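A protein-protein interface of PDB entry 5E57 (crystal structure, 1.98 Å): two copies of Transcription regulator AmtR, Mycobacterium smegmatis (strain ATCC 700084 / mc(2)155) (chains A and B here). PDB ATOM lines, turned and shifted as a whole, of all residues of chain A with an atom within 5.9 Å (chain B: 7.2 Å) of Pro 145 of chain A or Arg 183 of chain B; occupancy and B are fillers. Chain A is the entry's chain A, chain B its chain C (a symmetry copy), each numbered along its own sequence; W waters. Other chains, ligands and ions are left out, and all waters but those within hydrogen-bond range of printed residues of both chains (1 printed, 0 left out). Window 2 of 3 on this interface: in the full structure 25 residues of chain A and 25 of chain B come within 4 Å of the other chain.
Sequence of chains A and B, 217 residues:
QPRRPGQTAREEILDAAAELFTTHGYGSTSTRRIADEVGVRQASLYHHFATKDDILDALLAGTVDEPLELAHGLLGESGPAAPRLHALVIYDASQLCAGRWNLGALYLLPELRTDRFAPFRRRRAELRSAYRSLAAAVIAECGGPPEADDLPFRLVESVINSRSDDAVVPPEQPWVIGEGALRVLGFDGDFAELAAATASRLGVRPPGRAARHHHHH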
ATOM      1  N   ILE A 139      24.260  20.417 -23.076  1.00  0.00           N
ATOM      2  CA  ILE A 139      22.995  20.817 -22.527  1.00  0.00           C
ATOM      3  C   ILE A 139      22.139  21.616 -23.532  1.00  0.00           C
ATOM      4  O   ILE A 139      20.955  21.299 -23.701  1.00  0.00           O
ATOM      5  CB  ILE A 139      23.154  21.609 -21.213  1.00  0.00           C
ATOM      6  CG1 ILE A 139      23.592  20.655 -20.073  1.00  0.00           C
ATOM      7  CG2 ILE A 139      21.833  22.231 -20.796  1.00  0.00           C
ATOM      8  CD1 ILE A 139      24.194  21.381 -18.874  1.00  0.00           C
ATOM      9  N   GLY A 143      18.612  20.110 -24.950  1.00  0.00           N
ATOM     10  CA  GLY A 143      17.534  20.653 -24.188  1.00  0.00           C
ATOM     11  C   GLY A 143      17.544  20.081 -22.783  1.00  0.00           C
ATOM     12  O   GLY A 143      16.488  19.831 -22.214  1.00  0.00           O
ATOM     13  N   GLY A 144      18.739  19.906 -22.201  1.00  0.00           N
ATOM     14  CA  GLY A 144      18.868  19.298 -20.858  1.00  0.00           C
ATOM     15  C   GLY A 144      18.897  20.348 -19.747  1.00  0.00           C
ATOM     16  O   GLY A 144      18.620  21.506 -19.997  1.00  0.00           O
ATOM     17  N   PRO A 145      19.234  19.939 -18.503  1.00  0.00           N
ATOM     18  CA  PRO A 145      19.162  20.857 -17.358  1.00  0.00           C
ATOM     19  C   PRO A 145      20.338  21.808 -17.207  1.00  0.00           C
ATOM     20  O   PRO A 145      21.433  21.396 -16.904  1.00  0.00           O
ATOM     21  CB  PRO A 145      19.037  19.913 -16.163  1.00  0.00           C
ATOM     22  CG  PRO A 145      19.729  18.648 -16.603  1.00  0.00           C
ATOM     23  CD  PRO A 145      19.510  18.543 -18.102  1.00  0.00           C
ATOM     24  N   PRO A 146      20.109  23.114 -17.393  1.00  0.00           N
ATOM     25  CA  PRO A 146      21.243  24.020 -17.418  1.00  0.00           C
ATOM     26  C   PRO A 146      22.117  23.944 -16.177  1.00  0.00           C
ATOM     27  O   PRO A 146      23.319  24.219 -16.241  1.00  0.00           O
ATOM     28  CB  PRO A 146      20.591  25.420 -17.597  1.00  0.00           C
ATOM     29  CG  PRO A 146      19.173  25.241 -17.198  1.00  0.00           C
ATOM     30  CD  PRO A 146      18.838  23.828 -17.644  1.00  0.00           C
ATOM     31  N   GLU A 147      21.537  23.509 -15.072  1.00  0.00           N
ATOM     32  CA  GLU A 147      22.212  23.524 -13.805  1.00  0.00           C
ATOM     33  C   GLU A 147      23.210  22.364 -13.660  1.00  0.00           C
ATOM     34  O   GLU A 147      24.015  22.381 -12.749  1.00  0.00           O
ATOM     35  CB  GLU A 147      21.168  23.521 -12.665  1.00  0.00           C
ATOM     36  N   ALA A 148      23.206  21.392 -14.567  1.00  0.00           N
ATOM     37  CA  ALA A 148      24.019  20.216 -14.405  1.00  0.00           C
ATOM     38  C   ALA A 148      25.435  20.368 -14.931  1.00  0.00           C
ATOM     39  O   ALA A 148      26.178  19.395 -14.975  1.00  0.00           O
ATOM     40  CB  ALA A 148      23.348  19.040 -15.117  1.00  0.00           C
ATOM     41  N   ASP A 149      25.826  21.541 -15.404  1.00  0.00           N
ATOM     42  CA  ASP A 149      27.031  21.625 -16.182  1.00  0.00           C
ATOM     43  C   ASP A 149      28.336  21.311 -15.480  1.00  0.00           C
ATOM     44  O   ASP A 149      29.306  21.110 -16.154  1.00  0.00           O
ATOM     45  CB  ASP A 149      27.088  22.934 -16.988  1.00  0.00           C
ATOM     46  CG  ASP A 149      27.215  24.177 -16.153  1.00  0.00           C
ATOM     47  OD1 ASP A 149      27.323  24.124 -14.903  1.00  0.00           O
ATOM     48  OD2 ASP A 149      27.190  25.228 -16.807  1.00  0.00           O
ATOM     49  N   ARG A 183      24.340  11.377 -19.611  1.00  0.00           N
ATOM     50  CA  ARG A 183      22.955  11.410 -19.136  1.00  0.00           C
ATOM     51  C   ARG A 183      22.569  12.525 -18.231  1.00  0.00           C
ATOM     52  O   ARG A 183      21.407  13.005 -18.286  1.00  0.00           O
ATOM     53  CB  ARG A 183      22.534  10.111 -18.482  1.00  0.00           C
ATOM     54  CG  ARG A 183      22.541   9.011 -19.465  1.00  0.00           C
ATOM     55  CD  ARG A 183      22.053   7.773 -18.778  1.00  0.00           C
ATOM     56  NE  ARG A 183      22.261   6.672 -19.680  1.00  0.00           N
ATOM     57  CZ  ARG A 183      21.339   6.216 -20.469  1.00  0.00           C
ATOM     58  NH1 ARG A 183      20.090   6.739 -20.430  1.00  0.00           N
ATOM     59  NH2 ARG A 183      21.655   5.204 -21.297  1.00  0.00           N
ATOM     60  N   VAL A 184      23.491  12.998 -17.412  1.00  0.00           N
ATOM     61  CA  VAL A 184      23.117  14.038 -16.445  1.00  0.00           C
ATOM     62  C   VAL A 184      22.899  15.322 -17.174  1.00  0.00           C
ATOM     63  O   VAL A 184      22.271  16.256 -16.608  1.00  0.00           O
ATOM     64  CB  VAL A 184      24.136  14.346 -15.311  1.00  0.00           C
ATOM     65  CG1 VAL A 184      24.224  13.187 -14.400  1.00  0.00           C
ATOM     66  CG2 VAL A 184      25.520  14.691 -15.846  1.00  0.00           C
ATOM     67  N   LEU A 185      23.419  15.395 -18.393  1.00  0.00           N
ATOM     68  CA  LEU A 185      23.210  16.595 -19.208  1.00  0.00           C
ATOM     69  C   LEU A 185      21.993  16.527 -20.135  1.00  0.00           C
ATOM     70  O   LEU A 185      21.780  17.440 -20.892  1.00  0.00           O
ATOM     71  CB  LEU A 185      24.415  16.819 -20.077  1.00  0.00           C
ATOM     72  CG  LEU A 185      25.714  16.915 -19.322  1.00  0.00           C
ATOM     73  CD1 LEU A 185      26.834  17.088 -20.346  1.00  0.00           C
ATOM     74  CD2 LEU A 185      25.691  18.031 -18.303  1.00  0.00           C
ATOM     75  N   GLY A 186      21.259  15.420 -20.113  1.00  0.00           N
ATOM     76  CA  GLY A 186      20.041  15.254 -20.911  1.00  0.00           C
ATOM     77  C   GLY A 186      20.342  14.563 -22.206  1.00  0.00           C
ATOM     78  O   GLY A 186      19.494  14.455 -23.043  1.00  0.00           O
ATOM     79  N   PRO B 145      20.573   1.888 -17.706  1.00  0.00           N
ATOM     80  CA  PRO B 145      21.860   1.203 -17.741  1.00  0.00           C
ATOM     81  C   PRO B 145      22.242   0.470 -16.415  1.00  0.00           C
ATOM     82  O   PRO B 145      22.529   1.126 -15.411  1.00  0.00           O
ATOM     83  CB  PRO B 145      22.837   2.338 -18.064  1.00  0.00           C
ATOM     84  CG  PRO B 145      22.229   3.558 -17.465  1.00  0.00           C
ATOM     85  CD  PRO B 145      20.714   3.342 -17.480  1.00  0.00           C
ATOM     86  N   ALA B 148      25.203   1.620 -13.954  1.00  0.00           N
ATOM     87  CA  ALA B 148      25.210   2.931 -13.291  1.00  0.00           C
ATOM     88  C   ALA B 148      24.904   2.927 -11.822  1.00  0.00           C
ATOM     89  O   ALA B 148      24.719   4.007 -11.230  1.00  0.00           O
ATOM     90  CB  ALA B 148      24.243   3.906 -13.955  1.00  0.00           C
ATOM     91  N   LEU B 155      27.657  10.858  -6.866  1.00  0.00           N
ATOM     92  CA  LEU B 155      27.143  12.220  -7.103  1.00  0.00           C
ATOM     93  C   LEU B 155      26.886  12.962  -5.815  1.00  0.00           C
ATOM     94  O   LEU B 155      27.216  14.135  -5.679  1.00  0.00           O
ATOM     95  CB  LEU B 155      25.877  12.215  -8.006  1.00  0.00           C
ATOM     96  CG  LEU B 155      26.221  12.005  -9.491  1.00  0.00           C
ATOM     97  CD1 LEU B 155      25.084  11.411 -10.314  1.00  0.00           C
ATOM     98  CD2 LEU B 155      26.698  13.299 -10.156  1.00  0.00           C
ATOM     99  N   TRP B 175      19.220  19.541  -4.925  1.00  0.00           N
ATOM    100  CA  TRP B 175      18.212  19.182  -5.919  1.00  0.00           C
ATOM    101  C   TRP B 175      18.857  18.946  -7.251  1.00  0.00           C
ATOM    102  O   TRP B 175      18.430  18.086  -8.049  1.00  0.00           O
ATOM    103  CB  TRP B 175      17.124  20.228  -6.011  1.00  0.00           C
ATOM    104  CG  TRP B 175      16.541  20.481  -4.702  1.00  0.00           C
ATOM    105  CD1 TRP B 175      16.906  21.464  -3.806  1.00  0.00           C
ATOM    106  CD2 TRP B 175      15.487  19.732  -4.077  1.00  0.00           C
ATOM    107  NE1 TRP B 175      16.116  21.365  -2.664  1.00  0.00           N
ATOM    108  CE2 TRP B 175      15.220  20.338  -2.829  1.00  0.00           C
ATOM    109  CE3 TRP B 175      14.681  18.668  -4.490  1.00  0.00           C
ATOM    110  CZ2 TRP B 175      14.248  19.850  -1.945  1.00  0.00           C
ATOM    111  CZ3 TRP B 175      13.715  18.192  -3.598  1.00  0.00           C
ATOM    112  CH2 TRP B 175      13.519  18.797  -2.347  1.00  0.00           C
ATOM    113  N   VAL B 176      19.918  19.701  -7.490  1.00  0.00           N
ATOM    114  CA  VAL B 176      20.679  19.526  -8.696  1.00  0.00           C
ATOM    115  C   VAL B 176      21.327  18.145  -8.675  1.00  0.00           C
ATOM    116  O   VAL B 176      21.272  17.378  -9.644  1.00  0.00           O
ATOM    117  CB  VAL B 176      21.723  20.658  -8.806  1.00  0.00           C
ATOM    118  CG1 VAL B 176      22.725  20.372  -9.892  1.00  0.00           C
ATOM    119  CG2 VAL B 176      21.004  21.998  -9.047  1.00  0.00           C
ATOM    120  N   ILE B 177      21.942  17.805  -7.574  1.00  0.00           N
ATOM    121  CA  ILE B 177      22.426  16.430  -7.429  1.00  0.00           C
ATOM    122  C   ILE B 177      21.289  15.374  -7.547  1.00  0.00           C
ATOM    123  O   ILE B 177      21.472  14.272  -8.139  1.00  0.00           O
ATOM    124  CB  ILE B 177      23.086  16.255  -6.056  1.00  0.00           C
ATOM    125  CG1 ILE B 177      24.284  17.194  -5.919  1.00  0.00           C
ATOM    126  CG2 ILE B 177      23.477  14.798  -5.857  1.00  0.00           C
ATOM    127  CD1 ILE B 177      25.380  16.904  -6.872  1.00  0.00           C
ATOM    128  N   GLY B 178      20.172  15.679  -6.904  1.00  0.00           N
ATOM    129  CA  GLY B 178      18.921  14.816  -6.975  1.00  0.00           C
ATOM    130  C   GLY B 178      18.549  14.451  -8.389  1.00  0.00           C
ATOM    131  O   GLY B 178      18.440  13.244  -8.774  1.00  0.00           O
ATOM    132  N   GLU B 179      18.437  15.480  -9.240  1.00  0.00           N
ATOM    133  CA  GLU B 179      18.120  15.197 -10.624  1.00  0.00           C
ATOM    134  C   GLU B 179      19.195  14.366 -11.308  1.00  0.00           C
ATOM    135  O   GLU B 179      18.880  13.448 -12.071  1.00  0.00           O
ATOM    136  CB  GLU B 179      17.889  16.465 -11.448  1.00  0.00           C
ATOM    137  CG  GLU B 179      16.812  17.364 -10.874  1.00  0.00           C
ATOM    138  CD  GLU B 179      16.155  18.309 -11.897  1.00  0.00           C
ATOM    139  OE1 GLU B 179      16.602  18.333 -13.090  1.00  0.00           O
ATOM    140  OE2 GLU B 179      15.192  18.999 -11.446  1.00  0.00           O
ATOM    141  N   GLY B 180      20.474  14.722 -11.110  1.00  0.00           N
ATOM    142  CA  GLY B 180      21.511  14.022 -11.859  1.00  0.00           C
ATOM    143  C   GLY B 180      21.550  12.565 -11.447  1.00  0.00           C
ATOM    144  O   GLY B 180      21.816  11.687 -12.260  1.00  0.00           O
ATOM    145  N   ALA B 181      21.350  12.336 -10.148  1.00  0.00           N
ATOM    146  CA  ALA B 181      21.373  10.982  -9.572  1.00  0.00           C
ATOM    147  C   ALA B 181      20.371  10.098 -10.208  1.00  0.00           C
ATOM    148  O   ALA B 181      20.632   8.924 -10.409  1.00  0.00           O
ATOM    149  CB  ALA B 181      21.075  11.068  -8.073  1.00  0.00           C
ATOM    150  N   LEU B 182      19.231  10.663 -10.557  1.00  0.00           N
ATOM    151  CA  LEU B 182      18.218   9.889 -11.255  1.00  0.00           C
ATOM    152  C   LEU B 182      18.407   9.817 -12.742  1.00  0.00           C
ATOM    153  O   LEU B 182      18.186   8.741 -13.298  1.00  0.00           O
ATOM    154  CB  LEU B 182      16.804  10.307 -10.820  1.00  0.00           C
ATOM    155  CG  LEU B 182      16.646   9.329  -9.627  1.00  0.00           C
ATOM    156  CD1 LEU B 182      16.948  10.022  -8.295  1.00  0.00           C
ATOM    157  CD2 LEU B 182      15.345   8.559  -9.612  1.00  0.00           C
ATOM    158  N   ARG B 183      18.886  10.902 -13.387  1.00  0.00           N
ATOM    159  CA  ARG B 183      19.151  10.801 -14.852  1.00  0.00           C
ATOM    160  C   ARG B 183      20.127   9.714 -15.156  1.00  0.00           C
ATOM    161  O   ARG B 183      19.973   9.059 -16.178  1.00  0.00           O
ATOM    162  CB  ARG B 183      19.572  12.108 -15.523  1.00  0.00           C
ATOM    163  CG  ARG B 183      18.453  13.113 -15.673  1.00  0.00           C
ATOM    164  CD  ARG B 183      18.834  14.398 -16.436  1.00  0.00           C
ATOM    165  NE  ARG B 183      17.605  15.159 -16.649  1.00  0.00           N
ATOM    166  CZ  ARG B 183      17.149  16.148 -15.864  1.00  0.00           C
ATOM    167  NH1 ARG B 183      17.841  16.638 -14.823  1.00  0.00           N
ATOM    168  NH2 ARG B 183      15.952  16.670 -16.127  1.00  0.00           N
ATOM    169  N   VAL B 184      21.128   9.478 -14.289  1.00  0.00           N
ATOM    170  CA  VAL B 184      22.181   8.488 -14.641  1.00  0.00           C
ATOM    171  C   VAL B 184      21.670   7.111 -14.694  1.00  0.00           C
ATOM    172  O   VAL B 184      22.294   6.211 -15.297  1.00  0.00           O
ATOM    173  CB  VAL B 184      23.413   8.458 -13.687  1.00  0.00           C
ATOM    174  CG1 VAL B 184      24.320   9.626 -14.000  1.00  0.00           C
ATOM    175  CG2 VAL B 184      22.974   8.496 -12.240  1.00  0.00           C
ATOM    176  N   LEU B 185      20.538   6.930 -14.057  1.00  0.00           N
ATOM    177  CA  LEU B 185      19.924   5.604 -14.007  1.00  0.00           C
ATOM    178  C   LEU B 185      18.879   5.365 -15.105  1.00  0.00           C
ATOM    179  O   LEU B 185      18.239   4.309 -15.134  1.00  0.00           O
ATOM    180  CB  LEU B 185      19.236   5.471 -12.659  1.00  0.00           C
ATOM    181  CG  LEU B 185      20.122   5.823 -11.461  1.00  0.00           C
ATOM    182  CD1 LEU B 185      19.304   5.760 -10.151  1.00  0.00           C
ATOM    183  CD2 LEU B 185      21.297   4.882 -11.447  1.00  0.00           C
ATOM    184  N   GLY B 186      18.666   6.348 -15.980  1.00  0.00           N
ATOM    185  CA  GLY B 186      17.693   6.184 -17.058  1.00  0.00           C
ATOM    186  C   GLY B 186      16.325   6.685 -16.674  1.00  0.00           C
ATOM    187  O   GLY B 186      15.356   6.448 -17.394  1.00  0.00           O
ATOM    188  N   PHE B 187      16.215   7.381 -15.548  1.00  0.00           N
ATOM    189  CA  PHE B 187      14.968   8.037 -15.238  1.00  0.00           C
ATOM    190  C   PHE B 187      14.713   9.311 -16.083  1.00  0.00           C
ATOM    191  O   PHE B 187      15.512  10.226 -16.069  1.00  0.00           O
ATOM    192  CB  PHE B 187      14.939   8.372 -13.748  1.00  0.00           C
ATOM    193  CG  PHE B 187      13.659   8.993 -13.259  1.00  0.00           C
ATOM    194  CD1 PHE B 187      12.593   8.219 -12.830  1.00  0.00           C
ATOM    195  CD2 PHE B 187      13.555  10.352 -13.138  1.00  0.00           C
ATOM    196  CE1 PHE B 187      11.420   8.816 -12.342  1.00  0.00           C
ATOM    197  CE2 PHE B 187      12.407  10.950 -12.675  1.00  0.00           C
ATOM    198  CZ  PHE B 187      11.328  10.182 -12.262  1.00  0.00           C
ATOM    199  N   ASP B 188      13.573   9.380 -16.764  1.00  0.00           N
ATOM    200  CA  ASP B 188      13.133  10.621 -17.445  1.00  0.00           C
ATOM    201  C   ASP B 188      11.643  10.835 -17.220  1.00  0.00           C
ATOM    202  O   ASP B 188      10.935  11.131 -18.157  1.00  0.00           O
ATOM    203  CB  ASP B 188      13.446  10.624 -18.967  1.00  0.00           C
ATOM    204  N   GLY B 189      11.191  10.660 -15.977  1.00  0.00           N
ATOM    205  CA  GLY B 189       9.863  11.081 -15.533  1.00  0.00           C
ATOM    206  C   GLY B 189       9.829  12.582 -15.292  1.00  0.00           C
ATOM    207  O   GLY B 189      10.652  13.318 -15.838  1.00  0.00           O
ATOM    208  N   PHE B 191      10.313  15.724 -13.093  1.00  0.00           N
ATOM    209  CA  PHE B 191      11.168  16.080 -11.977  1.00  0.00           C
ATOM    210  C   PHE B 191      10.581  17.109 -11.028  1.00  0.00           C
ATOM    211  O   PHE B 191      10.983  17.145  -9.885  1.00  0.00           O
ATOM    212  CB  PHE B 191      12.539  16.535 -12.471  1.00  0.00           C
ATOM    213  CG  PHE B 191      13.374  15.427 -12.985  1.00  0.00           C
ATOM    214  CD1 PHE B 191      14.229  14.740 -12.140  1.00  0.00           C
ATOM    215  CD2 PHE B 191      13.294  15.048 -14.295  1.00  0.00           C
ATOM    216  CE1 PHE B 191      14.987  13.703 -12.603  1.00  0.00           C
ATOM    217  CE2 PHE B 191      14.055  14.016 -14.774  1.00  0.00           C
ATOM    218  CZ  PHE B 191      14.919  13.346 -13.920  1.00  0.00           C
HETATM  219  O   HOH W   1      20.852  16.032 -14.317  1.00  0.00           O
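The side-chain carboxylate of Glu 179 of chain B is in salt-bridge range of the guanidinium group of Arg 183 of chain B (2.7 Å).
Pro 145 of chain A touches Arg 183 of chain B.
CG1 of Val 176 of chain B touches O of Glu 147 of chain A, 3.7 Å away.
Arg 183 of chain A touches Pro 145 of chain B.
Arg 183 of chain B touches Arg 183 of chain A.
O of Val 184 of chain B touches CD of Arg 183 of chain A, 3.8 Å away.
Val 184 of chain A touches Gly 180 of chain B.
Val 184 of chain A touches Arg 183 of chain B.
Val 184 of chain B touches Val 184 of chain A.
Pro 145 of chain A touches just one residue of chain B: Arg 183.
Arg 183 of chain B touches three residues of chain A.
Of the printed residues of chain A, Pro 145 of chain B touches Arg 183.
Of the printed residues of chain A, Gly 180 of chain B touches Val 184.
Phe 191 of chain B touches none of the printed residues of chain A.
The nearest printed residue of chain B that does not touch Arg 183 of chain A is Gly 186 of chain B (4.2 Å).
Printed residues of chain B that touch a printed residue of chain A: Pro 145, Val 176, Gly 180, Arg 183 and Val 184.
Hydrophobic or aromatic side chains of chain B within 4 Å of the printed part of chain A: Pro 145, Val 176 and Val 184.
Along chain B the printed residues that touch a printed residue of chain A span positions 145 to 184.
Of the 12 printed residues of chain A, 4 touch a printed residue of chain B.
Hydrophobic or aromatic side chains of chain A within 4 Å of the printed part of chain B: Pro 145 and Val 184.
Along chain A the printed residues that touch a printed residue of chain B span positions 145 to 184.
Among the printed residues, no Asp or Glu carboxylate lies within 4 Å of a Lys or Arg side-chain nitrogen of the other chain.
Pro 145 of chain A touches Arg 183 of chain B, and with the chains exchanged Arg 183 of chain A touches Pro 145 of chain B.
Arg 183 of chain A touches its own counterpart, Arg 183 of chain B.
Arg 183 of chain A touches Val 184 of chain B, and with the chains exchanged Val 184 of chain A touches Arg 183 of chain B.
Val 184 of chain A touches its own counterpart, Val 184 of chain B.
Water W1 lies within hydrogen-bond range of the backbone carbonyl oxygen of Val 184 of chain A (2.7 Å), the guanidinium group of Arg 183 of chain B (3.1 Å) and the backbone NH of Gly 180 of chain B (3.5 Å).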
